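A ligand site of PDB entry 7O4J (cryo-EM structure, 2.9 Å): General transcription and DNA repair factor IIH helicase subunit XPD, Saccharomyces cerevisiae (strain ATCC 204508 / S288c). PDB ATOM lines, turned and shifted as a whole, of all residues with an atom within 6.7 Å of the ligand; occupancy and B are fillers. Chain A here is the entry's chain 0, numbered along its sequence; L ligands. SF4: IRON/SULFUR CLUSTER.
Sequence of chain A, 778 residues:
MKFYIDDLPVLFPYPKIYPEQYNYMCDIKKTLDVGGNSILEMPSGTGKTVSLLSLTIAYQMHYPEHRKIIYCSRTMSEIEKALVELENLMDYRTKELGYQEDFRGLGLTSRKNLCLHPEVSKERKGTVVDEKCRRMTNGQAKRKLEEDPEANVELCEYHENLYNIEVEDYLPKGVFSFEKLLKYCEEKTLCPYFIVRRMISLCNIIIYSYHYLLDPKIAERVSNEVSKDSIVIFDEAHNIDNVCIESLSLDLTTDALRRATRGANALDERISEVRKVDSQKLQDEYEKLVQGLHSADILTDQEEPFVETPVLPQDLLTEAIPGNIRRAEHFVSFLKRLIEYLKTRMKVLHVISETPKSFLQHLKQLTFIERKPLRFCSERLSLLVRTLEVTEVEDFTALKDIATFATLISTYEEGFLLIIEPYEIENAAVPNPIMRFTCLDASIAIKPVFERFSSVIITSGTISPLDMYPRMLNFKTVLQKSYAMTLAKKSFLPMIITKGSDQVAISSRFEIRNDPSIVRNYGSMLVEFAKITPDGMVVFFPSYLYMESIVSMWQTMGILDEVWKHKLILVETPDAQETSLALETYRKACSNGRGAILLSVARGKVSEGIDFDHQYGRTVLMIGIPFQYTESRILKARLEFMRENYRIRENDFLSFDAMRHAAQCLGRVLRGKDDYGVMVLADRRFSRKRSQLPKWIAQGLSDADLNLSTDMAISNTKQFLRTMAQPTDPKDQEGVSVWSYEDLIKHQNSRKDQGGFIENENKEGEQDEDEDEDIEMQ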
ATOM      1  N   ARG A 111      27.873   7.887 -19.323  1.00  0.00           N
ATOM      2  CA  ARG A 111      27.077   8.868 -20.034  1.00  0.00           C
ATOM      3  C   ARG A 111      25.929   8.201 -20.789  1.00  0.00           C
ATOM      4  O   ARG A 111      24.813   8.740 -20.843  1.00  0.00           O
ATOM      5  CB  ARG A 111      27.947   9.663 -21.003  1.00  0.00           C
ATOM      6  CG  ARG A 111      28.858  10.683 -20.343  1.00  0.00           C
ATOM      7  CD  ARG A 111      30.024  11.023 -21.242  1.00  0.00           C
ATOM      8  NE  ARG A 111      30.606  12.333 -20.937  1.00  0.00           N
ATOM      9  CZ  ARG A 111      31.852  12.546 -20.552  1.00  0.00           C
ATOM     10  NH1 ARG A 111      32.718  11.552 -20.413  1.00  0.00           N
ATOM     11  NH2 ARG A 111      32.260  13.788 -20.293  1.00  0.00           N
ATOM     12  N   LYS A 112      26.193   7.037 -21.380  1.00  0.00           N
ATOM     13  CA  LYS A 112      25.182   6.368 -22.193  1.00  0.00           C
ATOM     14  C   LYS A 112      23.897   6.143 -21.401  1.00  0.00           C
ATOM     15  O   LYS A 112      22.800   6.182 -21.979  1.00  0.00           O
ATOM     16  CB  LYS A 112      25.733   5.032 -22.698  1.00  0.00           C
ATOM     17  CG  LYS A 112      24.749   4.187 -23.495  1.00  0.00           C
ATOM     18  CD  LYS A 112      24.423   4.823 -24.832  1.00  0.00           C
ATOM     19  CE  LYS A 112      23.543   3.914 -25.666  1.00  0.00           C
ATOM     20  NZ  LYS A 112      24.306   2.767 -26.243  1.00  0.00           N
ATOM     21  N   LEU A 114      22.803   8.119 -19.022  1.00  0.00           N
ATOM     22  CA  LEU A 114      22.319   9.374 -18.455  1.00  0.00           C
ATOM     23  C   LEU A 114      22.374  10.540 -19.432  1.00  0.00           C
ATOM     24  O   LEU A 114      22.300  11.694 -19.000  1.00  0.00           O
ATOM     25  CB  LEU A 114      23.140   9.737 -17.206  1.00  0.00           C
ATOM     26  CG  LEU A 114      23.129   8.716 -16.056  1.00  0.00           C
ATOM     27  CD1 LEU A 114      24.231   9.031 -15.065  1.00  0.00           C
ATOM     28  CD2 LEU A 114      21.768   8.684 -15.378  1.00  0.00           C
ATOM     29  N   CYS A 115      22.485  10.276 -20.738  1.00  0.00           N
ATOM     30  CA  CYS A 115      22.560  11.351 -21.716  1.00  0.00           C
ATOM     31  C   CYS A 115      21.168  11.756 -22.176  1.00  0.00           C
ATOM     32  O   CYS A 115      20.394  10.920 -22.655  1.00  0.00           O
ATOM     33  CB  CYS A 115      23.415  10.924 -22.906  1.00  0.00           C
ATOM     34  SG  CYS A 115      23.749  12.245 -24.084  1.00  0.00           S
ATOM     35  N   LEU A 116      20.861  13.042 -22.048  1.00  0.00           N
ATOM     36  CA  LEU A 116      19.584  13.595 -22.483  1.00  0.00           C
ATOM     37  C   LEU A 116      19.692  14.361 -23.789  1.00  0.00           C
ATOM     38  O   LEU A 116      18.671  14.893 -24.261  1.00  0.00           O
ATOM     39  CB  LEU A 116      19.012  14.503 -21.393  1.00  0.00           C
ATOM     40  CG  LEU A 116      18.670  13.836 -20.057  1.00  0.00           C
ATOM     41  CD1 LEU A 116      18.272  14.881 -19.028  1.00  0.00           C
ATOM     42  CD2 LEU A 116      17.554  12.813 -20.239  1.00  0.00           C
ATOM     43  N   HIS A 117      20.867  14.451 -24.384  1.00  0.00           N
ATOM     44  CA  HIS A 117      21.011  15.165 -25.644  1.00  0.00           C
ATOM     45  C   HIS A 117      20.229  14.433 -26.734  1.00  0.00           C
ATOM     46  O   HIS A 117      20.410  13.224 -26.915  1.00  0.00           O
ATOM     47  CB  HIS A 117      22.487  15.258 -26.033  1.00  0.00           C
ATOM     48  CG  HIS A 117      22.775  16.300 -27.058  1.00  0.00           C
ATOM     49  ND1 HIS A 117      22.640  16.069 -28.412  1.00  0.00           N
ATOM     50  CD2 HIS A 117      23.195  17.584 -26.934  1.00  0.00           C
ATOM     51  CE1 HIS A 117      22.963  17.175 -29.071  1.00  0.00           C
ATOM     52  NE2 HIS A 117      23.306  18.109 -28.201  1.00  0.00           N
ATOM     53  N   VAL A 120      22.886  12.854 -29.246  1.00  0.00           N
ATOM     54  CA  VAL A 120      24.016  12.068 -28.773  1.00  0.00           C
ATOM     55  C   VAL A 120      23.582  10.822 -28.016  1.00  0.00           C
ATOM     56  O   VAL A 120      24.392   9.879 -27.900  1.00  0.00           O
ATOM     57  CB  VAL A 120      24.956  12.923 -27.900  1.00  0.00           C
ATOM     58  CG1 VAL A 120      26.060  12.069 -27.300  1.00  0.00           C
ATOM     59  CG2 VAL A 120      25.546  14.061 -28.718  1.00  0.00           C
ATOM     60  N   SER A 121      22.356  10.762 -27.503  1.00  0.00           N
ATOM     61  CA  SER A 121      21.869   9.586 -26.796  1.00  0.00           C
ATOM     62  C   SER A 121      21.333   8.519 -27.740  1.00  0.00           C
ATOM     63  O   SER A 121      20.892   7.468 -27.269  1.00  0.00           O
ATOM     64  CB  SER A 121      20.766   9.995 -25.817  1.00  0.00           C
ATOM     65  OG  SER A 121      19.711  10.659 -26.478  1.00  0.00           O
ATOM     66  N   VAL A 129      29.404   8.006 -27.565  1.00  0.00           N
ATOM     67  CA  VAL A 129      28.671   8.965 -26.732  1.00  0.00           C
ATOM     68  C   VAL A 129      29.650   9.819 -25.944  1.00  0.00           C
ATOM     69  O   VAL A 129      29.492  11.035 -25.830  1.00  0.00           O
ATOM     70  CB  VAL A 129      27.697   8.218 -25.803  1.00  0.00           C
ATOM     71  CG1 VAL A 129      27.012   9.203 -24.868  1.00  0.00           C
ATOM     72  CG2 VAL A 129      26.666   7.460 -26.624  1.00  0.00           C
ATOM     73  N   ASP A 130      30.689   9.188 -25.376  1.00  0.00           N
ATOM     74  CA  ASP A 130      31.691   9.943 -24.634  1.00  0.00           C
ATOM     75  C   ASP A 130      32.411  10.930 -25.532  1.00  0.00           C
ATOM     76  O   ASP A 130      32.664  12.085 -25.133  1.00  0.00           O
ATOM     77  CB  ASP A 130      32.687   8.972 -23.993  1.00  0.00           C
ATOM     78  CG  ASP A 130      32.206   8.435 -22.664  1.00  0.00           C
ATOM     79  OD1 ASP A 130      30.973   8.294 -22.486  1.00  0.00           O
ATOM     80  OD2 ASP A 130      33.055   8.147 -21.791  1.00  0.00           O
ATOM     81  N   LYS A 132      31.377  12.470 -28.319  1.00  0.00           N
ATOM     82  CA  LYS A 132      30.541  13.608 -28.697  1.00  0.00           C
ATOM     83  C   LYS A 132      30.328  14.548 -27.521  1.00  0.00           C
ATOM     84  O   LYS A 132      30.389  15.772 -27.667  1.00  0.00           O
ATOM     85  CB  LYS A 132      29.209  13.120 -29.260  1.00  0.00           C
ATOM     86  CG  LYS A 132      29.311  12.608 -30.691  1.00  0.00           C
ATOM     87  CD  LYS A 132      28.068  11.863 -31.126  1.00  0.00           C
ATOM     88  CE  LYS A 132      27.949  11.825 -32.643  1.00  0.00           C
ATOM     89  NZ  LYS A 132      27.934  10.442 -33.175  1.00  0.00           N
ATOM     90  N   CYS A 133      30.075  13.991 -26.338  1.00  0.00           N
ATOM     91  CA  CYS A 133      29.919  14.831 -25.151  1.00  0.00           C
ATOM     92  C   CYS A 133      31.195  15.601 -24.860  1.00  0.00           C
ATOM     93  O   CYS A 133      31.153  16.776 -24.505  1.00  0.00           O
ATOM     94  CB  CYS A 133      29.520  13.972 -23.951  1.00  0.00           C
ATOM     95  SG  CYS A 133      29.550  14.857 -22.376  1.00  0.00           S
ATOM     96  N   ARG A 134      32.350  14.949 -25.006  1.00  0.00           N
ATOM     97  CA  ARG A 134      33.617  15.631 -24.788  1.00  0.00           C
ATOM     98  C   ARG A 134      33.810  16.772 -25.777  1.00  0.00           C
ATOM     99  O   ARG A 134      34.319  17.831 -25.409  1.00  0.00           O
ATOM    100  CB  ARG A 134      34.775  14.627 -24.884  1.00  0.00           C
ATOM    101  CG  ARG A 134      35.173  14.021 -23.548  1.00  0.00           C
ATOM    102  CD  ARG A 134      36.108  12.846 -23.719  1.00  0.00           C
ATOM    103  NE  ARG A 134      35.961  11.878 -22.643  1.00  0.00           N
ATOM    104  CZ  ARG A 134      35.980  10.555 -22.779  1.00  0.00           C
ATOM    105  NH1 ARG A 134      36.147  10.006 -23.979  1.00  0.00           N
ATOM    106  NH2 ARG A 134      35.833   9.773 -21.723  1.00  0.00           N
ATOM    107  N   MET A 136      31.578  18.680 -27.012  1.00  0.00           N
ATOM    108  CA  MET A 136      30.726  19.793 -26.614  1.00  0.00           C
ATOM    109  C   MET A 136      30.980  20.275 -25.201  1.00  0.00           C
ATOM    110  O   MET A 136      30.419  21.302 -24.798  1.00  0.00           O
ATOM    111  CB  MET A 136      29.253  19.383 -26.729  1.00  0.00           C
ATOM    112  CG  MET A 136      28.799  19.087 -28.150  1.00  0.00           C
ATOM    113  SD  MET A 136      27.054  18.653 -28.245  1.00  0.00           S
ATOM    114  CE  MET A 136      27.011  17.154 -27.259  1.00  0.00           C
ATOM    115  N   THR A 137      31.827  19.581 -24.429  1.00  0.00           N
ATOM    116  CA  THR A 137      32.050  19.925 -23.025  1.00  0.00           C
ATOM    117  C   THR A 137      33.519  20.023 -22.647  1.00  0.00           C
ATOM    118  O   THR A 137      33.816  20.457 -21.526  1.00  0.00           O
ATOM    119  CB  THR A 137      31.379  18.902 -22.105  1.00  0.00           C
ATOM    120  OG1 THR A 137      32.019  17.627 -22.248  1.00  0.00           O
ATOM    121  CG2 THR A 137      29.904  18.768 -22.429  1.00  0.00           C
ATOM    122  N   CYS A 156      26.138  21.692 -25.443  1.00  0.00           N
ATOM    123  CA  CYS A 156      25.043  20.942 -24.837  1.00  0.00           C
ATOM    124  C   CYS A 156      24.343  21.854 -23.846  1.00  0.00           C
ATOM    125  O   CYS A 156      24.945  22.264 -22.844  1.00  0.00           O
ATOM    126  CB  CYS A 156      25.562  19.677 -24.155  1.00  0.00           C
ATOM    127  SG  CYS A 156      24.249  18.567 -23.587  1.00  0.00           S
ATOM    128  N   GLU A 157      23.074  22.175 -24.119  1.00  0.00           N
ATOM    129  CA  GLU A 157      22.335  23.060 -23.228  1.00  0.00           C
ATOM    130  C   GLU A 157      22.299  22.517 -21.807  1.00  0.00           C
ATOM    131  O   GLU A 157      22.264  23.283 -20.840  1.00  0.00           O
ATOM    132  CB  GLU A 157      20.900  23.257 -23.746  1.00  0.00           C
ATOM    133  CG  GLU A 157      20.227  21.999 -24.260  1.00  0.00           C
ATOM    134  CD  GLU A 157      18.782  22.235 -24.657  1.00  0.00           C
ATOM    135  OE1 GLU A 157      18.452  23.379 -25.050  1.00  0.00           O
ATOM    136  OE2 GLU A 157      17.984  21.285 -24.598  1.00  0.00           O
ATOM    137  N   TYR A 158      22.309  21.192 -21.660  1.00  0.00           N
ATOM    138  CA  TYR A 158      22.288  20.588 -20.331  1.00  0.00           C
ATOM    139  C   TYR A 158      23.565  20.920 -19.561  1.00  0.00           C
ATOM    140  O   TYR A 158      23.513  21.320 -18.395  1.00  0.00           O
ATOM    141  CB  TYR A 158      22.111  19.066 -20.451  1.00  0.00           C
ATOM    142  CG  TYR A 158      20.836  18.663 -21.151  1.00  0.00           C
ATOM    143  CD1 TYR A 158      20.756  18.641 -22.547  1.00  0.00           C
ATOM    144  CD2 TYR A 158      19.702  18.296 -20.432  1.00  0.00           C
ATOM    145  CE1 TYR A 158      19.597  18.264 -23.188  1.00  0.00           C
ATOM    146  CE2 TYR A 158      18.543  17.919 -21.072  1.00  0.00           C
ATOM    147  CZ  TYR A 158      18.493  17.910 -22.449  1.00  0.00           C
ATOM    148  OH  TYR A 158      17.334  17.533 -23.090  1.00  0.00           O
ATOM    149  N   HIS A 159      24.722  20.745 -20.204  1.00  0.00           N
ATOM    150  CA  HIS A 159      25.988  21.054 -19.546  1.00  0.00           C
ATOM    151  C   HIS A 159      26.114  22.551 -19.258  1.00  0.00           C
ATOM    152  O   HIS A 159      26.636  22.931 -18.204  1.00  0.00           O
ATOM    153  CB  HIS A 159      27.150  20.587 -20.419  1.00  0.00           C
ATOM    154  CG  HIS A 159      28.499  20.822 -19.807  1.00  0.00           C
ATOM    155  ND1 HIS A 159      29.385  21.761 -20.296  1.00  0.00           N
ATOM    156  CD2 HIS A 159      29.106  20.244 -18.748  1.00  0.00           C
ATOM    157  CE1 HIS A 159      30.482  21.755 -19.564  1.00  0.00           C
ATOM    158  NE2 HIS A 159      30.337  20.838 -18.618  1.00  0.00           N
ATOM    159  N   LEU A 190      19.190  19.690 -17.508  1.00  0.00           N
ATOM    160  CA  LEU A 190      20.484  19.516 -16.872  1.00  0.00           C
ATOM    161  C   LEU A 190      21.023  18.121 -17.191  1.00  0.00           C
ATOM    162  O   LEU A 190      20.268  17.207 -17.528  1.00  0.00           O
ATOM    163  CB  LEU A 190      20.406  19.717 -15.357  1.00  0.00           C
ATOM    164  CG  LEU A 190      19.771  21.017 -14.886  1.00  0.00           C
ATOM    165  CD1 LEU A 190      19.559  21.005 -13.386  1.00  0.00           C
ATOM    166  CD2 LEU A 190      20.621  22.213 -15.302  1.00  0.00           C
ATOM    167  N   CYS A 191      22.337  17.980 -17.080  1.00  0.00           N
ATOM    168  CA  CYS A 191      22.991  16.708 -17.391  1.00  0.00           C
ATOM    169  C   CYS A 191      23.063  15.857 -16.135  1.00  0.00           C
ATOM    170  O   CYS A 191      23.784  16.232 -15.192  1.00  0.00           O
ATOM    171  CB  CYS A 191      24.381  16.939 -17.941  1.00  0.00           C
ATOM    172  SG  CYS A 191      25.269  15.415 -18.329  1.00  0.00           S
ATOM    173  N   PRO A 192      22.355  14.727 -16.061  1.00  0.00           N
ATOM    174  CA  PRO A 192      22.498  13.865 -14.864  1.00  0.00           C
ATOM    175  C   PRO A 192      23.908  13.354 -14.664  1.00  0.00           C
ATOM    176  O   PRO A 192      24.343  13.204 -13.519  1.00  0.00           O
ATOM    177  CB  PRO A 192      21.509  12.721 -15.126  1.00  0.00           C
ATOM    178  CG  PRO A 192      20.620  13.194 -16.229  1.00  0.00           C
ATOM    179  CD  PRO A 192      21.402  14.168 -17.030  1.00  0.00           C
ATOM    180  N   TYR A 193      24.641  13.070 -15.741  1.00  0.00           N
ATOM    181  CA  TYR A 193      26.003  12.556 -15.596  1.00  0.00           C
ATOM    182  C   TYR A 193      26.898  13.558 -14.899  1.00  0.00           C
ATOM    183  O   TYR A 193      27.622  13.210 -13.956  1.00  0.00           O
ATOM    184  CB  TYR A 193      26.571  12.201 -16.974  1.00  0.00           C
ATOM    185  CG  TYR A 193      28.014  11.746 -16.930  1.00  0.00           C
ATOM    186  CD1 TYR A 193      28.350  10.476 -16.487  1.00  0.00           C
ATOM    187  CD2 TYR A 193      29.036  12.588 -17.349  1.00  0.00           C
ATOM    188  CE1 TYR A 193      29.675  10.066 -16.444  1.00  0.00           C
ATOM    189  CE2 TYR A 193      30.355  12.188 -17.314  1.00  0.00           C
ATOM    190  CZ  TYR A 193      30.668  10.921 -16.864  1.00  0.00           C
ATOM    191  OH  TYR A 193      31.984  10.514 -16.824  1.00  0.00           O
ATOM    192  N   PHE A 194      26.869  14.818 -15.331  1.00  0.00           N
ATOM    193  CA  PHE A 194      27.710  15.838 -14.719  1.00  0.00           C
ATOM    194  C   PHE A 194      27.200  16.272 -13.359  1.00  0.00           C
ATOM    195  O   PHE A 194      27.999  16.730 -12.522  1.00  0.00           O
ATOM    196  CB  PHE A 194      27.824  17.050 -15.647  1.00  0.00           C
ATOM    197  CG  PHE A 194      28.915  16.921 -16.671  1.00  0.00           C
ATOM    198  CD1 PHE A 194      30.245  16.943 -16.290  1.00  0.00           C
ATOM    199  CD2 PHE A 194      28.610  16.772 -18.009  1.00  0.00           C
ATOM    200  CE1 PHE A 194      31.251  16.816 -17.224  1.00  0.00           C
ATOM    201  CE2 PHE A 194      29.611  16.655 -18.952  1.00  0.00           C
ATOM    202  CZ  PHE A 194      30.937  16.675 -18.557  1.00  0.00           C
HETATM  203 FE1  SF4 L   1      24.845  13.882 -22.967  1.00  0.00          FE
HETATM  204 FE2  SF4 L   1      25.107  16.594 -22.859  1.00  0.00          FE
HETATM  205 FE3  SF4 L   1      27.296  15.002 -22.462  1.00  0.00          FE
HETATM  206 FE4  SF4 L   1      25.318  15.122 -20.572  1.00  0.00          FE
HETATM  207  S1  SF4 L   1      26.678  16.822 -21.233  1.00  0.00           S
HETATM  208  S2  SF4 L   1      26.337  13.239 -21.362  1.00  0.00           S
HETATM  209  S3  SF4 L   1      23.463  15.337 -21.896  1.00  0.00           S
HETATM  210  S4  SF4 L   1      26.076  15.192 -24.375  1.00  0.00           S
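SG of Cys 191 lies close to N of Tyr 193 (3.5 Å). The side-chain sulfur (SG) of Cys 133 sits close to the guanidinium group (NE) of Arg 111. SD of Met 136 lies within hydrogen-bond range of NE2 of His 117, 3.8 Å away. SG of Cys 156 sits close to N of Tyr 158 (3.8 Å). The backbone NH of His 117 sits close to the side-chain sulfur of Cys 115. A ring nitrogen (ND1) of His 117 sits at hydrogen-bond distance from the backbone NH of Val 120. SG of Cys 191 sits close to N of Phe 194, 3.5 Å away. The side-chain hydroxyl (OH) of Tyr 158 is in hydrogen-bond range of the backbone carbonyl oxygen (O) of Leu 116, 3.2 Å away.
SG of Cys 133 is bound to FE3 of the ligand (2.3 Å). N of Leu 116 sits close to S3 of the ligand, at 3.5 Å. An iron atom (FE4) of the ligand is bound by the side-chain sulfur (SG) of Cys 191 (2.3 Å). FE2 of the ligand is bound by SG of Cys 156 (2.3 Å). The side-chain sulfur (SG) of Cys 115 binds an iron atom (FE1) of the ligand, 2.3 Å away. The backbone NH (N) of His 117 sits close to a sulfur (S3) of the ligand, at 3.7 Å.
Arg 111 touches the ligand (CG to S2, 3.7 Å). Met 136 touches the ligand (CE to S4, 3.6 Å). Thr 137 touches the ligand. CB of His 159 touches S1 of the ligand (3.9 Å). CE2 of Phe 194 touches S1 of the ligand, 3.7 Å away. Hydrophobic or aromatic side chains that line the ligand: His 117, Met 136, His 159 and Phe 194. 11 residues have an atom within 4 Å of the ligand: Arg 111, Cys 115, Leu 116, His 117, Cys 133, Met 136, Thr 137, Cys 156, His 159, Cys 191 and Phe 194. Along chain A the residues within 4 Å of the ligand span positions 111 to 194.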
